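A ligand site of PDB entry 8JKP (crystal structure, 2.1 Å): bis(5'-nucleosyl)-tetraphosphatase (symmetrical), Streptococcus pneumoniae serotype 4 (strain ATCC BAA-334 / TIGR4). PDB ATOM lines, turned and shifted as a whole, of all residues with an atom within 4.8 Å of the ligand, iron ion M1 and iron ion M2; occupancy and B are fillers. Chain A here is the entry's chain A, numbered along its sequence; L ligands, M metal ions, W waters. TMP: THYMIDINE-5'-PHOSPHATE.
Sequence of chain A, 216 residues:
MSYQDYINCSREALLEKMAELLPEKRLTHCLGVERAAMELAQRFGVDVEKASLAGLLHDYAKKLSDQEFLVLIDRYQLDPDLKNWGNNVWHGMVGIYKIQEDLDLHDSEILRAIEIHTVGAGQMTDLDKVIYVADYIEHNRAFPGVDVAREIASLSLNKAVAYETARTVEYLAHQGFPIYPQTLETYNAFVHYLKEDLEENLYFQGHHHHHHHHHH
Of the 19 residues printed, 4 come within 4 Å of iron ion M1.
Iron ion M1 is bound by NE2 of His 29 (2.0 Å), water W4 (2.0 Å), NE2 of His 58 (2.0 Å), water W1 (2.1 Å), OD1 of Asp 135 (2.1 Å) and OD2 of Asp 59 (2.1 Å).
Iron ion M1 has six donor atoms within binding distance.
A ring nitrogen (NE2) of His 117 sits close to the side-chain hydroxyl (OG1) of Thr 118 (3.3 Å).
O of Asn 88 lies within hydrogen-bond range of ND1 of His 91 (3.3 Å).
OD2 of Asp 59 sits close to NH2 of Arg 26, 2.9 Å away.
The side-chain hydroxyl (OG1) of Thr 183 sits close to the backbone carbonyl oxygen (O) of Tyr 180 (3.5 Å).
O of Leu 172 sits at hydrogen-bond distance from N of Phe 177.
Water W1 bridges O3P of the ligand (2.8 Å) and NH2 of Arg 26 (3.3 Å).
Water W4 bridges the side-chain carboxylate (OD2) of Asp 135 (2.8 Å) and an oxygen (O3P) of the ligand (3.0 Å).
Water W7 lies within hydrogen-bond range of the side-chain amino group of Lys 62 (2.9 Å) and an oxygen (O3P) of the ligand (2.9 Å).
Water W3 lies within hydrogen-bond range of O1P of the ligand (3.0 Å) and OD2 of Asp 135 (3.2 Å).
Water W2 lies within hydrogen-bond range of OD2 of Asp 135, O of His 117 and O1P of the ligand.
NE2 of His 117 is bound to iron ion M2 (2.0 Å).
Iron ion M2 is bound by water W7 (2.0 Å).
Iron ion M2 is bound by NE2 of His 91.
Iron ion M2 is bound by water W4 (2.1 Å).
OD1 of Asp 59 binds iron ion M2, 2.1 Å away.
Iron ion M2 is bound by O2P of the ligand (2.1 Å).
Iron ion M2 has six donor atoms within binding distance.
OG1 of Thr 118 lies close to O2P of the ligand (2.7 Å).
OG1 of Thr 183 sits at hydrogen-bond distance from O4 of the ligand, at 2.8 Å.
O2 of the ligand lies within hydrogen-bond range of ND2 of Asn 88 (3.0 Å).
O4 of the ligand lies within hydrogen-bond range of N of Tyr 180 (3.2 Å).
Merely in contact with iron ion M2: Thr 118 (3.7 Å).
Of the 19 residues printed, 4 come within 4 Å of iron ion M2.
The nearest printed residue that does not touch iron ion M2 is His 58 (4.02 Å).
Merely in contact with the ligand: Lys 62 (3.7 Å), Thr 168 (3.7 Å), Leu 172 (3.4 Å) and Phe 177 (3.9 Å).
Hydrophobic or aromatic side chains that line the ligand: His 91, His 117, Leu 172, Phe 177 and Tyr 180.
Within 4 Å of the ligand: Lys 62, Asn 88, His 91, His 117, Thr 118, Asp 135, Thr 168, Leu 172, Phe 177, Tyr 180 and Thr 183.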
ATOM      1  N   ARG A  26      17.197  18.264 -14.029  1.00  0.00           N
ATOM      2  CA  ARG A  26      15.877  18.038 -13.419  1.00  0.00           C
ATOM      3  C   ARG A  26      15.821  16.733 -12.605  1.00  0.00           C
ATOM      4  O   ARG A  26      15.237  16.692 -11.517  1.00  0.00           O
ATOM      5  CB  ARG A  26      14.765  18.073 -14.490  1.00  0.00           C
ATOM      6  CG  ARG A  26      13.330  17.986 -13.923  1.00  0.00           C
ATOM      7  CD  ARG A  26      12.990  19.094 -12.923  1.00  0.00           C
ATOM      8  NE  ARG A  26      13.176  20.412 -13.521  1.00  0.00           N
ATOM      9  CZ  ARG A  26      12.827  21.572 -12.970  1.00  0.00           C
ATOM     10  NH1 ARG A  26      13.059  22.692 -13.639  1.00  0.00           N
ATOM     11  NH2 ARG A  26      12.262  21.628 -11.767  1.00  0.00           N
ATOM     12  N   HIS A  29      17.755  17.342  -9.478  1.00  0.00           N
ATOM     13  CA  HIS A  29      16.810  18.076  -8.628  1.00  0.00           C
ATOM     14  C   HIS A  29      15.901  17.117  -7.891  1.00  0.00           C
ATOM     15  O   HIS A  29      15.786  17.218  -6.676  1.00  0.00           O
ATOM     16  CB  HIS A  29      15.996  19.117  -9.427  1.00  0.00           C
ATOM     17  CG  HIS A  29      14.819  19.691  -8.685  1.00  0.00           C
ATOM     18  ND1 HIS A  29      14.939  20.526  -7.611  1.00  0.00           N
ATOM     19  CD2 HIS A  29      13.481  19.561  -8.911  1.00  0.00           C
ATOM     20  CE1 HIS A  29      13.731  20.897  -7.193  1.00  0.00           C
ATOM     21  NE2 HIS A  29      12.814  20.330  -7.969  1.00  0.00           N
ATOM     22  N   VAL A  33      15.440  16.482  -3.934  1.00  0.00           N
ATOM     23  CA  VAL A  33      14.176  16.613  -3.213  1.00  0.00           C
ATOM     24  C   VAL A  33      13.886  15.320  -2.445  1.00  0.00           C
ATOM     25  O   VAL A  33      13.432  15.378  -1.314  1.00  0.00           O
ATOM     26  CB  VAL A  33      12.971  17.041  -4.113  1.00  0.00           C
ATOM     27  CG1 VAL A  33      11.696  17.191  -3.294  1.00  0.00           C
ATOM     28  CG2 VAL A  33      13.233  18.368  -4.830  1.00  0.00           C
ATOM     29  N   HIS A  58       7.950  14.360  -7.497  1.00  0.00           N
ATOM     30  CA  HIS A  58       7.129  15.585  -7.535  1.00  0.00           C
ATOM     31  C   HIS A  58       7.187  16.311  -8.905  1.00  0.00           C
ATOM     32  O   HIS A  58       6.180  16.854  -9.346  1.00  0.00           O
ATOM     33  CB  HIS A  58       7.498  16.549  -6.413  1.00  0.00           C
ATOM     34  CG  HIS A  58       8.741  17.316  -6.702  1.00  0.00           C
ATOM     35  ND1 HIS A  58       9.973  16.721  -6.769  1.00  0.00           N
ATOM     36  CD2 HIS A  58       8.937  18.619  -7.045  1.00  0.00           C
ATOM     37  CE1 HIS A  58      10.880  17.632  -7.075  1.00  0.00           C
ATOM     38  NE2 HIS A  58      10.283  18.809  -7.268  1.00  0.00           N
ATOM     39  N   ASP A  59       8.343  16.246  -9.569  1.00  0.00           N
ATOM     40  CA  ASP A  59       8.578  16.887 -10.871  1.00  0.00           C
ATOM     41  C   ASP A  59       8.640  15.897 -12.052  1.00  0.00           C
ATOM     42  O   ASP A  59       9.158  16.233 -13.112  1.00  0.00           O
ATOM     43  CB  ASP A  59       9.840  17.763 -10.853  1.00  0.00           C
ATOM     44  CG  ASP A  59       9.579  19.199 -10.385  1.00  0.00           C
ATOM     45  OD1 ASP A  59       8.401  19.644 -10.258  1.00  0.00           O
ATOM     46  OD2 ASP A  59      10.564  19.940 -10.061  1.00  0.00           O
ATOM     47  N   LYS A  62       7.210  17.166 -15.391  1.00  0.00           N
ATOM     48  CA  LYS A  62       7.692  18.514 -15.706  1.00  0.00           C
ATOM     49  C   LYS A  62       7.818  18.775 -17.220  1.00  0.00           C
ATOM     50  O   LYS A  62       7.571  19.896 -17.657  1.00  0.00           O
ATOM     51  CB  LYS A  62       9.023  18.797 -14.996  1.00  0.00           C
ATOM     52  CG  LYS A  62       9.576  20.215 -15.117  1.00  0.00           C
ATOM     53  CD  LYS A  62       8.802  21.254 -14.307  1.00  0.00           C
ATOM     54  CE  LYS A  62       9.472  22.610 -14.439  1.00  0.00           C
ATOM     55  NZ  LYS A  62       9.064  23.573 -13.380  1.00  0.00           N
ATOM     56  N   ASN A  88       3.604  25.325 -15.218  1.00  0.00           N
ATOM     57  CA  ASN A  88       3.838  25.686 -13.815  1.00  0.00           C
ATOM     58  C   ASN A  88       2.733  25.131 -12.907  1.00  0.00           C
ATOM     59  O   ASN A  88       3.031  24.446 -11.918  1.00  0.00           O
ATOM     60  CB  ASN A  88       3.997  27.209 -13.641  1.00  0.00           C
ATOM     61  CG  ASN A  88       5.285  27.752 -14.286  1.00  0.00           C
ATOM     62  OD1 ASN A  88       6.164  26.991 -14.686  1.00  0.00           O
ATOM     63  ND2 ASN A  88       5.405  29.061 -14.372  1.00  0.00           N
ATOM     64  N   HIS A  91       2.074  20.652 -14.067  1.00  0.00           N
ATOM     65  CA  HIS A  91       2.994  19.508 -13.835  1.00  0.00           C
ATOM     66  C   HIS A  91       2.734  18.774 -12.513  1.00  0.00           C
ATOM     67  O   HIS A  91       2.883  17.554 -12.454  1.00  0.00           O
ATOM     68  CB  HIS A  91       4.473  19.868 -14.083  1.00  0.00           C
ATOM     69  CG  HIS A  91       5.125  20.639 -12.968  1.00  0.00           C
ATOM     70  ND1 HIS A  91       5.003  22.006 -12.837  1.00  0.00           N
ATOM     71  CD2 HIS A  91       5.948  20.248 -11.959  1.00  0.00           C
ATOM     72  CE1 HIS A  91       5.718  22.420 -11.797  1.00  0.00           C
ATOM     73  NE2 HIS A  91       6.312  21.370 -11.231  1.00  0.00           N
ATOM     74  N   HIS A 117       2.342  20.600  -4.833  1.00  0.00           N
ATOM     75  CA  HIS A 117       3.751  20.907  -4.510  1.00  0.00           C
ATOM     76  C   HIS A 117       4.179  22.309  -4.980  1.00  0.00           C
ATOM     77  O   HIS A 117       5.073  22.893  -4.379  1.00  0.00           O
ATOM     78  CB  HIS A 117       4.726  19.813  -5.002  1.00  0.00           C
ATOM     79  CG  HIS A 117       5.185  19.986  -6.420  1.00  0.00           C
ATOM     80  ND1 HIS A 117       4.558  19.376  -7.470  1.00  0.00           N
ATOM     81  CD2 HIS A 117       6.222  20.692  -6.944  1.00  0.00           C
ATOM     82  CE1 HIS A 117       5.164  19.714  -8.599  1.00  0.00           C
ATOM     83  NE2 HIS A 117       6.202  20.511  -8.315  1.00  0.00           N
ATOM     84  N   THR A 118       3.534  22.843  -6.011  1.00  0.00           N
ATOM     85  CA  THR A 118       3.861  24.183  -6.547  1.00  0.00           C
ATOM     86  C   THR A 118       3.019  25.261  -5.852  1.00  0.00           C
ATOM     87  O   THR A 118       3.555  26.262  -5.400  1.00  0.00           O
ATOM     88  CB  THR A 118       3.640  24.268  -8.080  1.00  0.00           C
ATOM     89  OG1 THR A 118       4.332  23.203  -8.723  1.00  0.00           O
ATOM     90  CG2 THR A 118       4.089  25.610  -8.678  1.00  0.00           C
ATOM     91  N   VAL A 119       1.712  25.016  -5.747  1.00  0.00           N
ATOM     92  CA  VAL A 119       0.752  26.062  -5.388  1.00  0.00           C
ATOM     93  C   VAL A 119       0.323  25.988  -3.922  1.00  0.00           C
ATOM     94  O   VAL A 119      -0.240  26.944  -3.401  1.00  0.00           O
ATOM     95  CB  VAL A 119      -0.485  26.051  -6.360  1.00  0.00           C
ATOM     96  CG1 VAL A 119      -0.031  26.333  -7.785  1.00  0.00           C
ATOM     97  CG2 VAL A 119      -1.251  24.721  -6.321  1.00  0.00           C
ATOM     98  N   ASP A 135      11.321  20.733  -1.919  1.00  0.00           N
ATOM     99  CA  ASP A 135      11.454  21.263  -3.286  1.00  0.00           C
ATOM    100  C   ASP A 135      12.323  22.534  -3.332  1.00  0.00           C
ATOM    101  O   ASP A 135      13.186  22.698  -4.214  1.00  0.00           O
ATOM    102  CB  ASP A 135      10.049  21.551  -3.828  1.00  0.00           C
ATOM    103  CG  ASP A 135      10.038  21.898  -5.304  1.00  0.00           C
ATOM    104  OD1 ASP A 135      10.900  21.422  -6.118  1.00  0.00           O
ATOM    105  OD2 ASP A 135       9.109  22.630  -5.689  1.00  0.00           O
ATOM    106  N   THR A 168       7.647  33.413  -3.244  1.00  0.00           N
ATOM    107  CA  THR A 168       7.117  33.070  -4.569  1.00  0.00           C
ATOM    108  C   THR A 168       6.110  34.106  -5.053  1.00  0.00           C
ATOM    109  O   THR A 168       6.216  34.560  -6.173  1.00  0.00           O
ATOM    110  CB  THR A 168       6.533  31.654  -4.553  1.00  0.00           C
ATOM    111  OG1 THR A 168       7.590  30.762  -4.213  1.00  0.00           O
ATOM    112  CG2 THR A 168       5.944  31.225  -5.905  1.00  0.00           C
ATOM    113  N   LEU A 172       6.694  36.407  -8.308  1.00  0.00           N
ATOM    114  CA  LEU A 172       5.749  36.416  -9.438  1.00  0.00           C
ATOM    115  C   LEU A 172       5.208  37.819  -9.741  1.00  0.00           C
ATOM    116  O   LEU A 172       5.129  38.223 -10.908  1.00  0.00           O
ATOM    117  CB  LEU A 172       4.607  35.401  -9.238  1.00  0.00           C
ATOM    118  CG  LEU A 172       5.027  33.919  -9.202  1.00  0.00           C
ATOM    119  CD1 LEU A 172       3.875  33.033  -8.737  1.00  0.00           C
ATOM    120  CD2 LEU A 172       5.562  33.452 -10.554  1.00  0.00           C
ATOM    121  N   PHE A 177       4.043  38.155 -13.489  1.00  0.00           N
ATOM    122  CA  PHE A 177       3.516  36.861 -13.903  1.00  0.00           C
ATOM    123  C   PHE A 177       2.183  36.538 -13.233  1.00  0.00           C
ATOM    124  O   PHE A 177       2.008  36.850 -12.060  1.00  0.00           O
ATOM    125  CB  PHE A 177       4.549  35.780 -13.596  1.00  0.00           C
ATOM    126  CG  PHE A 177       4.586  34.712 -14.618  1.00  0.00           C
ATOM    127  CD1 PHE A 177       5.177  34.946 -15.867  1.00  0.00           C
ATOM    128  CD2 PHE A 177       3.976  33.485 -14.374  1.00  0.00           C
ATOM    129  CE1 PHE A 177       5.190  33.952 -16.843  1.00  0.00           C
ATOM    130  CE2 PHE A 177       3.985  32.476 -15.346  1.00  0.00           C
ATOM    131  CZ  PHE A 177       4.596  32.713 -16.584  1.00  0.00           C
ATOM    132  N   PRO A 178       1.240  35.903 -13.969  1.00  0.00           N
ATOM    133  CA  PRO A 178      -0.022  35.519 -13.304  1.00  0.00           C
ATOM    134  C   PRO A 178       0.236  34.614 -12.105  1.00  0.00           C
ATOM    135  O   PRO A 178       1.218  33.861 -12.089  1.00  0.00           O
ATOM    136  CB  PRO A 178      -0.801  34.761 -14.393  1.00  0.00           C
ATOM    137  CG  PRO A 178      -0.162  35.161 -15.688  1.00  0.00           C
ATOM    138  CD  PRO A 178       1.267  35.472 -15.377  1.00  0.00           C
ATOM    139  N   ILE A 179      -0.610  34.747 -11.099  1.00  0.00           N
ATOM    140  CA  ILE A 179      -0.486  33.969  -9.868  1.00  0.00           C
ATOM    141  C   ILE A 179      -1.720  33.113  -9.684  1.00  0.00           C
ATOM    142  O   ILE A 179      -2.842  33.628  -9.548  1.00  0.00           O
ATOM    143  CB  ILE A 179      -0.315  34.874  -8.619  1.00  0.00           C
ATOM    144  CG1 ILE A 179       1.003  35.655  -8.672  1.00  0.00           C
ATOM    145  CG2 ILE A 179      -0.439  34.058  -7.321  1.00  0.00           C
ATOM    146  CD1 ILE A 179       1.003  36.923  -7.845  1.00  0.00           C
ATOM    147  N   TYR A 180      -1.517  31.799  -9.652  1.00  0.00           N
ATOM    148  CA  TYR A 180      -2.636  30.885  -9.511  1.00  0.00           C
ATOM    149  C   TYR A 180      -3.391  31.160  -8.195  1.00  0.00           C
ATOM    150  O   TYR A 180      -2.748  31.320  -7.175  1.00  0.00           O
ATOM    151  CB  TYR A 180      -2.145  29.446  -9.567  1.00  0.00           C
ATOM    152  CG  TYR A 180      -3.257  28.463  -9.743  1.00  0.00           C
ATOM    153  CD1 TYR A 180      -4.003  28.426 -10.936  1.00  0.00           C
ATOM    154  CD2 TYR A 180      -3.576  27.563  -8.724  1.00  0.00           C
ATOM    155  CE1 TYR A 180      -5.041  27.521 -11.101  1.00  0.00           C
ATOM    156  CE2 TYR A 180      -4.605  26.642  -8.897  1.00  0.00           C
ATOM    157  CZ  TYR A 180      -5.336  26.642 -10.077  1.00  0.00           C
ATOM    158  OH  TYR A 180      -6.355  25.745 -10.242  1.00  0.00           O
ATOM    159  N   THR A 183      -2.509  29.423  -4.836  1.00  0.00           N
ATOM    160  CA  THR A 183      -1.270  29.945  -4.229  1.00  0.00           C
ATOM    161  C   THR A 183      -1.564  31.022  -3.172  1.00  0.00           C
ATOM    162  O   THR A 183      -0.950  31.044  -2.096  1.00  0.00           O
ATOM    163  CB  THR A 183      -0.308  30.512  -5.295  1.00  0.00           C
ATOM    164  OG1 THR A 183       0.023  29.467  -6.212  1.00  0.00           O
ATOM    165  CG2 THR A 183       0.987  31.104  -4.678  1.00  0.00           C
HETATM  166  P   TMP L   1       7.925  24.579  -8.711  1.00  0.00           P
HETATM  167  O1P TMP L   1       7.695  25.096  -7.299  1.00  0.00           O
HETATM  168  O2P TMP L   1       7.012  23.412  -9.107  1.00  0.00           O
HETATM  169  O3P TMP L   1       9.391  24.333  -9.018  1.00  0.00           O
HETATM  170  O5' TMP L   1       7.462  25.847  -9.590  1.00  0.00           O
HETATM  171  C5' TMP L   1       7.874  26.045 -10.934  1.00  0.00           C
HETATM  172  C4' TMP L   1       7.527  27.465 -11.382  1.00  0.00           C
HETATM  173  O4' TMP L   1       6.127  27.720 -11.225  1.00  0.00           O
HETATM  174  C3' TMP L   1       8.272  28.543 -10.624  1.00  0.00           C
HETATM  175  O3' TMP L   1       9.171  29.167 -11.524  1.00  0.00           O
HETATM  176  C2' TMP L   1       7.231  29.570 -10.205  1.00  0.00           C
HETATM  177  C1' TMP L   1       5.962  29.099 -10.917  1.00  0.00           C
HETATM  178  N1  TMP L   1       4.715  29.362 -10.176  1.00  0.00           N
HETATM  179  C2  TMP L   1       3.674  29.976 -10.912  1.00  0.00           C
HETATM  180  O2  TMP L   1       3.847  30.235 -12.115  1.00  0.00           O
HETATM  181  N3  TMP L   1       2.497  30.295 -10.389  1.00  0.00           N
HETATM  182  C4  TMP L   1       2.263  30.021  -9.116  1.00  0.00           C
HETATM  183  O4  TMP L   1       1.158  30.330  -8.675  1.00  0.00           O
HETATM  184  C5  TMP L   1       3.337  29.376  -8.289  1.00  0.00           C
HETATM  185  C5M TMP L   1       3.154  29.049  -6.839  1.00  0.00           C
HETATM  186  C6  TMP L   1       4.562  29.076  -8.878  1.00  0.00           C
HETATM  187 FE    FE M   1      10.838  20.612  -8.060  1.00  0.00          FE
HETATM  188 FE    FE M   2       7.488  21.396  -9.572  1.00  0.00          FE
HETATM  189  O   HOH W   1      11.487  22.464  -8.669  1.00  0.00           O
HETATM  190  O   HOH W   2       7.396  24.143  -4.394  1.00  0.00           O
HETATM  191  O   HOH W   3      10.211  25.667  -5.854  1.00  0.00           O
HETATM  192  O   HOH W   4       8.998  21.453  -8.174  1.00  0.00           O
HETATM  193  O   HOH W   5       6.925  27.632  -6.983  1.00  0.00           O
HETATM  194  O   HOH W   6      11.200  26.056  -9.485  1.00  0.00           O
HETATM  195  O   HOH W   7       8.845  22.129 -10.895  1.00  0.00           O
